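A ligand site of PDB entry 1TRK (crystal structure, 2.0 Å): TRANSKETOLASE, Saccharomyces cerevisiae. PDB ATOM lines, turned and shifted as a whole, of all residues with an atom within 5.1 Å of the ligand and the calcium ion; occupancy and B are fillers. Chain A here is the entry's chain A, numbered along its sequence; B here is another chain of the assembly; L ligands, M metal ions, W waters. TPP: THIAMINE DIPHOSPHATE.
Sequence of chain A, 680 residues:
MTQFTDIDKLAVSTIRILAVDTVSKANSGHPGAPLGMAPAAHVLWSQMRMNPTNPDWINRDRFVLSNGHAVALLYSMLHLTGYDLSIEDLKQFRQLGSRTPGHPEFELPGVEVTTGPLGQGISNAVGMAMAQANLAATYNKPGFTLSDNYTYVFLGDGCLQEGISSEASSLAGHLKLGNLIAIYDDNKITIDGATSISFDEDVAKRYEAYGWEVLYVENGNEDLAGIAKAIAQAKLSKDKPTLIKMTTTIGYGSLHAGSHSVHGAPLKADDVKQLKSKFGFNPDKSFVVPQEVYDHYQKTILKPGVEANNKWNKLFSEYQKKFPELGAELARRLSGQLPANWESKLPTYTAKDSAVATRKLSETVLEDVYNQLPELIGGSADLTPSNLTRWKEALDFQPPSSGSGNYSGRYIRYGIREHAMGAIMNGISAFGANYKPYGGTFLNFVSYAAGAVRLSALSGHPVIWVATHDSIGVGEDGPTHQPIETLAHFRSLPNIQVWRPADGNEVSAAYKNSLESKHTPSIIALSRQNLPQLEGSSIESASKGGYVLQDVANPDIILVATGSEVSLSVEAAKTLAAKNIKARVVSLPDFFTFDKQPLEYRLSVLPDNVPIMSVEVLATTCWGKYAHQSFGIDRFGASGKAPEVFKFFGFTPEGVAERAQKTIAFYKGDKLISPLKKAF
The side-chain carboxylate of Asp 185 is in hydrogen-bond range of the side-chain amide nitrogen of Asn 187.
The side-chain carboxylate (OE2) of Glu 162 sits close to the side-chain carboxylate (OE1) of Glu 418 of chain B, 2.6 Å away.
The side-chain hydroxyl (OH) of Tyr 448 of chain B lies within hydrogen-bond range of the backbone carbonyl oxygen (O) of Leu 118.
OG1 of Thr 190 sits at hydrogen-bond distance from OD1 of Asp 382 of chain B (2.7 Å).
OD2 of Asp 382 of chain B is in hydrogen-bond range of N of Ile 191.
N of Asp 157 lies within hydrogen-bond range of O1A of the ligand (3.5 Å).
A ring nitrogen (ND1) of His 263 sits at hydrogen-bond distance from an oxygen (O2B) of the ligand, 2.8 Å away.
An oxygen (O3B) of the ligand sits at hydrogen-bond distance from a ring nitrogen (NE2) of His 69 (2.9 Å).
The backbone carbonyl oxygen (O) of Gly 116 lies within hydrogen-bond range of a nitrogen (N4') of the ligand.
N of Leu 118 sits at hydrogen-bond distance from N3' of the ligand.
An oxygen (O1A) of the ligand sits at hydrogen-bond distance from the backbone NH of Gly 158 (3.2 Å).
Of the 28 residues printed, 3 come within 4 Å of the calcium ion.
N1' of the ligand lies close to OE2 of Glu 418 of chain B, at 2.9 Å.
CB of Ala 33 touches O3B of the ligand (3.5 Å).
CA of Pro 117 touches N3' of the ligand, at 3.6 Å.
C of Gly 156 touches O1A of the ligand, at 3.7 Å.
OE2 of Glu 162 touches CM2 of the ligand (3.3 Å).
Thr 190 touches the ligand (CG2 to O2A, 3.3 Å).
Ile 191 touches the ligand (CD1 to C4, 3.6 Å).
CD1 of Ile 250 touches O2B of the ligand, 3.4 Å away.
OD2 of Asp 382 of chain B touches C6 of the ligand (3.3 Å).
Ile 416 of chain B touches the ligand.
CD2 of Phe 445 of chain B touches N1' of the ligand (3.5 Å).
Tyr 448 of chain B touches the ligand.
NE2 of His 481 of chain B touches N4' of the ligand, at 3.5 Å.
Hydrophobic or aromatic side chains within 4 Å of the ligand: Ala 33, His 69, Leu 118, Ile 191, Ile 250, His 263, Ile 416 of chain B, Phe 445 of chain B, Tyr 448 of chain B and His 481 of chain B.
21 residues have an atom within 4 Å of the ligand: Ala 33, His 69, Gly 116, Pro 117, Leu 118, Gly 156, Asp 157, Gly 158, Glu 162, Asn 187, Ile 189, Thr 190, Ile 191, Ile 250, His 263, Asp 382 of chain B, Ile 416 of chain B, Glu 418 of chain B, Phe 445 of chain B, Tyr 448 of chain B and His 481 of chain B.
Water W2 lies within hydrogen-bond range of O of Asp 185 (3.0 Å) and N of Asp 157 (3.0 Å).
Water W1 lies within hydrogen-bond range of O3B of the ligand (2.4 Å), OD2 of Asp 185 (2.8 Å) and OD1 of Asn 67 (3.0 Å).
Water W4 lies within hydrogen-bond range of an oxygen (O1A) of the ligand, the side-chain sulfur of Cys 159 and the backbone NH of Gly 156.
Water W3 lies within hydrogen-bond range of the backbone carbonyl oxygen (O) of His 263, an oxygen (O2B) of the ligand and the backbone NH (N) of Ala 33.
Water W6 lies within hydrogen-bond range of a ring nitrogen (NE2) of His 481 of chain B (3.2 Å) and a nitrogen (N4') of the ligand (3.5 Å).
Water W5 bridges O of Ala 381 of chain B and OE2 of Glu 418 of chain B.
The calcium ion is bound by water W2 (2.2 Å), O1B of the ligand (2.3 Å), OD1 of Asn 187 (2.3 Å), OD2 of Asp 157 (2.4 Å), O of Ile 189 (2.4 Å) and O2A of the ligand (2.5 Å).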
ATOM      1  N   ALA A  33      21.076 -34.477  -5.737  1.00  0.00           N
ATOM      2  CA  ALA A  33      21.714 -34.822  -4.478  1.00  0.00           C
ATOM      3  C   ALA A  33      21.237 -36.166  -3.898  1.00  0.00           C
ATOM      4  O   ALA A  33      22.104 -36.856  -3.333  1.00  0.00           O
ATOM      5  CB  ALA A  33      21.463 -33.728  -3.435  1.00  0.00           C
ATOM      6  N   ASN A  67      19.605 -30.174   3.657  1.00  0.00           N
ATOM      7  CA  ASN A  67      19.366 -29.888   2.251  1.00  0.00           C
ATOM      8  C   ASN A  67      18.044 -30.523   1.845  1.00  0.00           C
ATOM      9  O   ASN A  67      17.984 -31.400   0.999  1.00  0.00           O
ATOM     10  CB  ASN A  67      20.519 -30.430   1.390  1.00  0.00           C
ATOM     11  CG  ASN A  67      21.111 -31.776   1.781  1.00  0.00           C
ATOM     12  OD1 ASN A  67      21.905 -32.329   1.034  1.00  0.00           O
ATOM     13  ND2 ASN A  67      20.855 -32.430   2.870  1.00  0.00           N
ATOM     14  N   HIS A  69      15.684 -30.281  -0.246  1.00  0.00           N
ATOM     15  CA  HIS A  69      15.222 -30.581  -1.582  1.00  0.00           C
ATOM     16  C   HIS A  69      15.640 -31.948  -2.051  1.00  0.00           C
ATOM     17  O   HIS A  69      15.147 -32.355  -3.088  1.00  0.00           O
ATOM     18  CB  HIS A  69      15.720 -29.588  -2.636  1.00  0.00           C
ATOM     19  CG  HIS A  69      17.204 -29.465  -2.601  1.00  0.00           C
ATOM     20  ND1 HIS A  69      17.891 -28.658  -1.811  1.00  0.00           N
ATOM     21  CD2 HIS A  69      18.104 -30.250  -3.305  1.00  0.00           C
ATOM     22  CE1 HIS A  69      19.159 -28.913  -1.957  1.00  0.00           C
ATOM     23  NE2 HIS A  69      19.266 -29.873  -2.848  1.00  0.00           N
ATOM     24  N   GLY A 116      13.922 -27.497   3.964  1.00  0.00           N
ATOM     25  CA  GLY A 116      13.610 -26.987   2.619  1.00  0.00           C
ATOM     26  C   GLY A 116      14.181 -25.566   2.428  1.00  0.00           C
ATOM     27  O   GLY A 116      15.114 -25.355   1.625  1.00  0.00           O
ATOM     28  N   PRO A 117      13.691 -24.540   3.175  1.00  0.00           N
ATOM     29  CA  PRO A 117      14.411 -23.289   3.423  1.00  0.00           C
ATOM     30  C   PRO A 117      15.836 -23.580   3.923  1.00  0.00           C
ATOM     31  O   PRO A 117      16.065 -24.142   5.012  1.00  0.00           O
ATOM     32  CB  PRO A 117      13.574 -22.551   4.466  1.00  0.00           C
ATOM     33  CG  PRO A 117      12.211 -23.112   4.189  1.00  0.00           C
ATOM     34  CD  PRO A 117      12.542 -24.593   4.060  1.00  0.00           C
ATOM     35  N   LEU A 118      16.830 -23.218   3.126  1.00  0.00           N
ATOM     36  CA  LEU A 118      18.233 -23.536   3.454  1.00  0.00           C
ATOM     37  C   LEU A 118      18.793 -22.886   4.715  1.00  0.00           C
ATOM     38  O   LEU A 118      18.458 -21.765   5.078  1.00  0.00           O
ATOM     39  CB  LEU A 118      19.117 -23.181   2.272  1.00  0.00           C
ATOM     40  CG  LEU A 118      18.782 -23.849   0.966  1.00  0.00           C
ATOM     41  CD1 LEU A 118      19.512 -23.184  -0.192  1.00  0.00           C
ATOM     42  CD2 LEU A 118      19.152 -25.330   1.087  1.00  0.00           C
ATOM     43  N   GLY A 156      24.274 -29.297   2.287  1.00  0.00           N
ATOM     44  CA  GLY A 156      24.870 -29.010   0.994  1.00  0.00           C
ATOM     45  C   GLY A 156      25.486 -27.618   0.937  1.00  0.00           C
ATOM     46  O   GLY A 156      25.649 -26.911   1.953  1.00  0.00           O
ATOM     47  N   ASP A 157      25.895 -27.188  -0.242  1.00  0.00           N
ATOM     48  CA  ASP A 157      26.480 -25.842  -0.404  1.00  0.00           C
ATOM     49  C   ASP A 157      25.618 -24.651  -0.052  1.00  0.00           C
ATOM     50  O   ASP A 157      26.057 -23.714   0.619  1.00  0.00           O
ATOM     51  CB  ASP A 157      26.952 -25.626  -1.821  1.00  0.00           C
ATOM     52  CG  ASP A 157      28.070 -26.593  -2.235  1.00  0.00           C
ATOM     53  OD1 ASP A 157      29.193 -26.410  -1.739  1.00  0.00           O
ATOM     54  OD2 ASP A 157      27.818 -27.525  -3.024  1.00  0.00           O
ATOM     55  N   GLY A 158      24.358 -24.643  -0.506  1.00  0.00           N
ATOM     56  CA  GLY A 158      23.395 -23.605  -0.115  1.00  0.00           C
ATOM     57  C   GLY A 158      23.257 -23.346   1.386  1.00  0.00           C
ATOM     58  O   GLY A 158      23.248 -22.201   1.858  1.00  0.00           O
ATOM     59  N   CYS A 159      23.175 -24.434   2.151  1.00  0.00           N
ATOM     60  CA  CYS A 159      23.139 -24.352   3.622  1.00  0.00           C
ATOM     61  C   CYS A 159      24.367 -23.641   4.196  1.00  0.00           C
ATOM     62  O   CYS A 159      24.246 -22.841   5.128  1.00  0.00           O
ATOM     63  CB  CYS A 159      23.082 -25.729   4.291  1.00  0.00           C
ATOM     64  SG  CYS A 159      21.449 -26.562   4.156  1.00  0.00           S
ATOM     65  N   GLU A 162      24.173 -19.638   3.590  1.00  0.00           N
ATOM     66  CA  GLU A 162      23.230 -18.937   4.427  1.00  0.00           C
ATOM     67  C   GLU A 162      23.827 -18.531   5.777  1.00  0.00           C
ATOM     68  O   GLU A 162      24.400 -19.358   6.489  1.00  0.00           O
ATOM     69  CB  GLU A 162      22.041 -19.800   4.680  1.00  0.00           C
ATOM     70  CG  GLU A 162      21.086 -19.880   3.498  1.00  0.00           C
ATOM     71  CD  GLU A 162      20.300 -18.572   3.207  1.00  0.00           C
ATOM     72  OE1 GLU A 162      20.407 -17.579   3.928  1.00  0.00           O
ATOM     73  OE2 GLU A 162      19.537 -18.579   2.243  1.00  0.00           O
ATOM     74  N   ASP A 185      27.819 -32.540   1.706  1.00  0.00           N
ATOM     75  CA  ASP A 185      27.817 -33.010   0.332  1.00  0.00           C
ATOM     76  C   ASP A 185      28.608 -32.053  -0.579  1.00  0.00           C
ATOM     77  O   ASP A 185      28.111 -31.115  -1.225  1.00  0.00           O
ATOM     78  CB  ASP A 185      26.361 -33.160  -0.124  1.00  0.00           C
ATOM     79  CG  ASP A 185      26.185 -33.609  -1.607  1.00  0.00           C
ATOM     80  OD1 ASP A 185      27.085 -34.225  -2.167  1.00  0.00           O
ATOM     81  OD2 ASP A 185      25.148 -33.356  -2.208  1.00  0.00           O
ATOM     82  N   ASN A 187      29.657 -31.155  -3.630  1.00  0.00           N
ATOM     83  CA  ASN A 187      29.574 -31.558  -5.020  1.00  0.00           C
ATOM     84  C   ASN A 187      29.899 -30.505  -6.059  1.00  0.00           C
ATOM     85  O   ASN A 187      29.710 -30.748  -7.247  1.00  0.00           O
ATOM     86  CB  ASN A 187      28.161 -32.160  -5.332  1.00  0.00           C
ATOM     87  CG  ASN A 187      26.990 -31.242  -5.089  1.00  0.00           C
ATOM     88  OD1 ASN A 187      27.150 -30.037  -4.920  1.00  0.00           O
ATOM     89  ND2 ASN A 187      25.761 -31.734  -5.012  1.00  0.00           N
ATOM     90  N   LYS A 188      30.356 -29.300  -5.707  1.00  0.00           N
ATOM     91  CA  LYS A 188      30.798 -28.261  -6.648  1.00  0.00           C
ATOM     92  C   LYS A 188      29.817 -27.525  -7.535  1.00  0.00           C
ATOM     93  O   LYS A 188      30.215 -26.638  -8.298  1.00  0.00           O
ATOM     94  CB  LYS A 188      31.892 -28.795  -7.594  1.00  0.00           C
ATOM     95  CG  LYS A 188      33.302 -28.629  -7.059  1.00  0.00           C
ATOM     96  CD  LYS A 188      33.615 -29.586  -5.936  1.00  0.00           C
ATOM     97  CE  LYS A 188      35.009 -29.310  -5.409  1.00  0.00           C
ATOM     98  NZ  LYS A 188      35.290 -30.087  -4.216  1.00  0.00           N
ATOM     99  N   ILE A 189      28.543 -27.839  -7.362  1.00  0.00           N
ATOM    100  CA  ILE A 189      27.435 -27.299  -8.136  1.00  0.00           C
ATOM    101  C   ILE A 189      26.322 -26.704  -7.248  1.00  0.00           C
ATOM    102  O   ILE A 189      25.925 -27.256  -6.229  1.00  0.00           O
ATOM    103  CB  ILE A 189      26.928 -28.529  -9.009  1.00  0.00           C
ATOM    104  CG1 ILE A 189      27.729 -28.560 -10.333  1.00  0.00           C
ATOM    105  CG2 ILE A 189      25.386 -28.514  -9.175  1.00  0.00           C
ATOM    106  CD1 ILE A 189      27.427 -27.481 -11.398  1.00  0.00           C
ATOM    107  N   THR A 190      25.774 -25.556  -7.585  1.00  0.00           N
ATOM    108  CA  THR A 190      24.535 -25.093  -6.958  1.00  0.00           C
ATOM    109  C   THR A 190      23.545 -24.715  -8.065  1.00  0.00           C
ATOM    110  O   THR A 190      23.811 -25.045  -9.238  1.00  0.00           O
ATOM    111  CB  THR A 190      24.729 -23.846  -6.030  1.00  0.00           C
ATOM    112  OG1 THR A 190      25.150 -22.776  -6.869  1.00  0.00           O
ATOM    113  CG2 THR A 190      25.723 -24.071  -4.886  1.00  0.00           C
ATOM    114  N   ILE A 191      22.410 -24.040  -7.870  1.00  0.00           N
ATOM    115  CA  ILE A 191      21.526 -23.757  -9.022  1.00  0.00           C
ATOM    116  C   ILE A 191      22.182 -22.934 -10.147  1.00  0.00           C
ATOM    117  O   ILE A 191      21.995 -23.271 -11.323  1.00  0.00           O
ATOM    118  CB  ILE A 191      20.246 -23.054  -8.523  1.00  0.00           C
ATOM    119  CG1 ILE A 191      19.438 -24.069  -7.764  1.00  0.00           C
ATOM    120  CG2 ILE A 191      19.430 -22.417  -9.644  1.00  0.00           C
ATOM    121  CD1 ILE A 191      18.115 -23.552  -7.246  1.00  0.00           C
ATOM    122  N   ILE A 250      27.303 -34.631  -8.211  1.00  0.00           N
ATOM    123  CA  ILE A 250      25.855 -34.447  -8.319  1.00  0.00           C
ATOM    124  C   ILE A 250      25.247 -35.344  -9.409  1.00  0.00           C
ATOM    125  O   ILE A 250      25.832 -35.512 -10.485  1.00  0.00           O
ATOM    126  CB  ILE A 250      25.530 -32.928  -8.584  1.00  0.00           C
ATOM    127  CG1 ILE A 250      24.045 -32.768  -8.276  1.00  0.00           C
ATOM    128  CG2 ILE A 250      25.944 -32.444  -9.977  1.00  0.00           C
ATOM    129  CD1 ILE A 250      23.547 -31.346  -7.908  1.00  0.00           C
ATOM    130  N   HIS A 263      20.173 -30.797 -11.064  1.00  0.00           N
ATOM    131  CA  HIS A 263      19.775 -30.386  -9.709  1.00  0.00           C
ATOM    132  C   HIS A 263      18.261 -30.460  -9.386  1.00  0.00           C
ATOM    133  O   HIS A 263      17.850 -30.961  -8.332  1.00  0.00           O
ATOM    134  CB  HIS A 263      20.285 -28.935  -9.446  1.00  0.00           C
ATOM    135  CG  HIS A 263      19.617 -28.202  -8.260  1.00  0.00           C
ATOM    136  ND1 HIS A 263      19.967 -28.320  -6.981  1.00  0.00           N
ATOM    137  CD2 HIS A 263      18.505 -27.381  -8.331  1.00  0.00           C
ATOM    138  CE1 HIS A 263      19.115 -27.624  -6.271  1.00  0.00           C
ATOM    139  NE2 HIS A 263      18.253 -27.078  -7.088  1.00  0.00           N
ATOM    140  N   ALA B 381      20.061 -14.353  -6.141  1.00  0.00           N
ATOM    141  CA  ALA B 381      20.624 -15.123  -5.056  1.00  0.00           C
ATOM    142  C   ALA B 381      20.593 -16.648  -5.377  1.00  0.00           C
ATOM    143  O   ALA B 381      19.868 -17.507  -4.819  1.00  0.00           O
ATOM    144  CB  ALA B 381      19.834 -14.762  -3.776  1.00  0.00           C
ATOM    145  N   ASP B 382      21.412 -16.992  -6.392  1.00  0.00           N
ATOM    146  CA  ASP B 382      21.483 -18.335  -6.986  1.00  0.00           C
ATOM    147  C   ASP B 382      20.199 -18.835  -7.630  1.00  0.00           C
ATOM    148  O   ASP B 382      19.951 -20.015  -7.758  1.00  0.00           O
ATOM    149  CB  ASP B 382      21.944 -19.328  -5.913  1.00  0.00           C
ATOM    150  CG  ASP B 382      22.443 -20.658  -6.454  1.00  0.00           C
ATOM    151  OD1 ASP B 382      23.448 -20.638  -7.161  1.00  0.00           O
ATOM    152  OD2 ASP B 382      21.804 -21.678  -6.154  1.00  0.00           O
ATOM    153  N   LEU B 383      19.336 -17.979  -8.137  1.00  0.00           N
ATOM    154  CA  LEU B 383      18.108 -18.423  -8.781  1.00  0.00           C
ATOM    155  C   LEU B 383      17.928 -17.811 -10.152  1.00  0.00           C
ATOM    156  O   LEU B 383      16.804 -17.696 -10.656  1.00  0.00           O
ATOM    157  CB  LEU B 383      16.906 -18.068  -7.920  1.00  0.00           C
ATOM    158  CG  LEU B 383      16.587 -19.040  -6.822  1.00  0.00           C
ATOM    159  CD1 LEU B 383      15.605 -18.409  -5.822  1.00  0.00           C
ATOM    160  CD2 LEU B 383      16.114 -20.360  -7.493  1.00  0.00           C
ATOM    161  N   ILE B 416      23.663 -18.042  -2.296  1.00  0.00           N
ATOM    162  CA  ILE B 416      22.448 -18.218  -1.533  1.00  0.00           C
ATOM    163  C   ILE B 416      22.605 -17.409  -0.253  1.00  0.00           C
ATOM    164  O   ILE B 416      22.791 -17.876   0.869  1.00  0.00           O
ATOM    165  CB  ILE B 416      22.208 -19.701  -1.222  1.00  0.00           C
ATOM    166  CG1 ILE B 416      22.087 -20.574  -2.492  1.00  0.00           C
ATOM    167  CG2 ILE B 416      20.806 -19.819  -0.650  1.00  0.00           C
ATOM    168  CD1 ILE B 416      23.421 -21.226  -2.957  1.00  0.00           C
ATOM    169  N   GLU B 418      20.471 -14.146   0.665  1.00  0.00           N
ATOM    170  CA  GLU B 418      19.456 -13.091   0.513  1.00  0.00           C
ATOM    171  C   GLU B 418      19.608 -11.881   1.456  1.00  0.00           C
ATOM    172  O   GLU B 418      19.437 -10.746   1.021  1.00  0.00           O
ATOM    173  CB  GLU B 418      18.067 -13.595   0.730  1.00  0.00           C
ATOM    174  CG  GLU B 418      17.709 -14.790  -0.142  1.00  0.00           C
ATOM    175  CD  GLU B 418      18.172 -16.175   0.346  1.00  0.00           C
ATOM    176  OE1 GLU B 418      18.676 -16.250   1.465  1.00  0.00           O
ATOM    177  OE2 GLU B 418      17.994 -17.153  -0.371  1.00  0.00           O
ATOM    178  N   PHE B 442      13.121 -16.033  -4.633  1.00  0.00           N
ATOM    179  CA  PHE B 442      11.701 -16.345  -4.495  1.00  0.00           C
ATOM    180  C   PHE B 442      11.112 -15.403  -3.447  1.00  0.00           C
ATOM    181  O   PHE B 442      11.739 -15.043  -2.424  1.00  0.00           O
ATOM    182  CB  PHE B 442      11.479 -17.797  -4.000  1.00  0.00           C
ATOM    183  CG  PHE B 442      11.965 -18.856  -4.987  1.00  0.00           C
ATOM    184  CD1 PHE B 442      11.986 -18.599  -6.356  1.00  0.00           C
ATOM    185  CD2 PHE B 442      12.315 -20.114  -4.547  1.00  0.00           C
ATOM    186  CE1 PHE B 442      12.318 -19.614  -7.249  1.00  0.00           C
ATOM    187  CE2 PHE B 442      12.656 -21.123  -5.454  1.00  0.00           C
ATOM    188  CZ  PHE B 442      12.653 -20.887  -6.803  1.00  0.00           C
ATOM    189  N   PHE B 445      11.448 -16.079   0.401  1.00  0.00           N
ATOM    190  CA  PHE B 445      12.717 -15.923   1.060  1.00  0.00           C
ATOM    191  C   PHE B 445      13.249 -14.491   1.009  1.00  0.00           C
ATOM    192  O   PHE B 445      14.275 -14.195   1.621  1.00  0.00           O
ATOM    193  CB  PHE B 445      13.748 -16.910   0.443  1.00  0.00           C
ATOM    194  CG  PHE B 445      13.257 -18.377   0.491  1.00  0.00           C
ATOM    195  CD1 PHE B 445      12.786 -18.914   1.673  1.00  0.00           C
ATOM    196  CD2 PHE B 445      13.265 -19.129  -0.667  1.00  0.00           C
ATOM    197  CE1 PHE B 445      12.298 -20.214   1.705  1.00  0.00           C
ATOM    198  CE2 PHE B 445      12.783 -20.420  -0.627  1.00  0.00           C
ATOM    199  CZ  PHE B 445      12.297 -20.962   0.549  1.00  0.00           C
ATOM    200  N   TYR B 448      13.974 -13.651   4.452  1.00  0.00           N
ATOM    201  CA  TYR B 448      15.294 -13.893   5.050  1.00  0.00           C
ATOM    202  C   TYR B 448      16.088 -12.578   5.176  1.00  0.00           C
ATOM    203  O   TYR B 448      16.990 -12.444   6.004  1.00  0.00           O
ATOM    204  CB  TYR B 448      16.086 -14.878   4.187  1.00  0.00           C
ATOM    205  CG  TYR B 448      16.046 -16.348   4.609  1.00  0.00           C
ATOM    206  CD1 TYR B 448      14.858 -17.017   4.877  1.00  0.00           C
ATOM    207  CD2 TYR B 448      17.243 -17.020   4.731  1.00  0.00           C
ATOM    208  CE1 TYR B 448      14.867 -18.360   5.268  1.00  0.00           C
ATOM    209  CE2 TYR B 448      17.274 -18.337   5.124  1.00  0.00           C
ATOM    210  CZ  TYR B 448      16.086 -18.998   5.382  1.00  0.00           C
ATOM    211  OH  TYR B 448      16.149 -20.311   5.732  1.00  0.00           O
ATOM    212  N   HIS B 481       7.595 -23.210   0.579  1.00  0.00           N
ATOM    213  CA  HIS B 481       8.003 -22.299  -0.516  1.00  0.00           C
ATOM    214  C   HIS B 481       6.891 -21.372  -1.045  1.00  0.00           C
ATOM    215  O   HIS B 481       7.114 -20.514  -1.895  1.00  0.00           O
ATOM    216  CB  HIS B 481       8.528 -23.103  -1.714  1.00  0.00           C
ATOM    217  CG  HIS B 481       9.911 -23.701  -1.457  1.00  0.00           C
ATOM    218  ND1 HIS B 481      10.334 -24.513  -0.471  1.00  0.00           N
ATOM    219  CD2 HIS B 481      11.012 -23.417  -2.246  1.00  0.00           C
ATOM    220  CE1 HIS B 481      11.609 -24.705  -0.600  1.00  0.00           C
ATOM    221  NE2 HIS B 481      11.986 -24.046  -1.667  1.00  0.00           N
HETATM  222  N1' TPP L   1      16.743 -19.793  -0.412  1.00  0.00           N
HETATM  223  C2' TPP L   1      16.422 -20.554   0.670  1.00  0.00           C
HETATM  224  CM2 TPP L   1      16.596 -19.968   1.992  1.00  0.00           C
HETATM  225  N3' TPP L   1      15.908 -21.747   0.571  1.00  0.00           N
HETATM  226  C4' TPP L   1      15.809 -22.294  -0.672  1.00  0.00           C
HETATM  227  N4' TPP L   1      15.363 -23.535  -0.719  1.00  0.00           N
HETATM  228  C5' TPP L   1      16.149 -21.543  -1.856  1.00  0.00           C
HETATM  229  C6' TPP L   1      16.605 -20.286  -1.664  1.00  0.00           C
HETATM  230  C7' TPP L   1      16.075 -22.130  -3.244  1.00  0.00           C
HETATM  231  N3  TPP L   1      17.123 -23.240  -3.335  1.00  0.00           N
HETATM  232  C2  TPP L   1      16.865 -24.547  -3.180  1.00  0.00           C
HETATM  233  S1  TPP L   1      18.200 -25.522  -3.437  1.00  0.00           S
HETATM  234  C5  TPP L   1      19.144 -24.100  -3.788  1.00  0.00           C
HETATM  235  C4  TPP L   1      18.383 -22.979  -3.691  1.00  0.00           C
HETATM  236  CM4 TPP L   1      18.821 -21.594  -4.068  1.00  0.00           C
HETATM  237  C6  TPP L   1      20.550 -24.158  -4.315  1.00  0.00           C
HETATM  238  C7  TPP L   1      21.256 -25.465  -4.430  1.00  0.00           C
HETATM  239  O7  TPP L   1      21.837 -25.709  -3.122  1.00  0.00           O
HETATM  240  PA  TPP L   1      22.791 -26.947  -2.912  1.00  0.00           P
HETATM  241  O1A TPP L   1      22.661 -27.187  -1.453  1.00  0.00           O
HETATM  242  O2A TPP L   1      24.116 -26.609  -3.462  1.00  0.00           O
HETATM  243  O3A TPP L   1      22.160 -28.111  -3.828  1.00  0.00           O
HETATM  244  PB  TPP L   1      22.516 -29.575  -4.306  1.00  0.00           P
HETATM  245  O1B TPP L   1      23.959 -29.520  -4.551  1.00  0.00           O
HETATM  246  O2B TPP L   1      21.702 -29.864  -5.499  1.00  0.00           O
HETATM  247  O3B TPP L   1      22.147 -30.343  -3.090  1.00  0.00           O
HETATM  248 CA    CA M   1      25.847 -28.365  -4.090  1.00  0.00          CA
HETATM  249  O   HOH W   1      23.494 -31.276  -1.288  1.00  0.00           O
HETATM  250  O   HOH W   2      25.788 -29.481  -2.189  1.00  0.00           O
HETATM  251  O   HOH W   3      19.345 -31.645  -6.005  1.00  0.00           O
HETATM  252  O   HOH W   4      22.071 -27.041   1.339  1.00  0.00           O
HETATM  253  O   HOH W   5      17.594 -17.481  -3.262  1.00  0.00           O
HETATM  254  O   HOH W   6      14.153 -26.206  -2.541  1.00  0.00           O
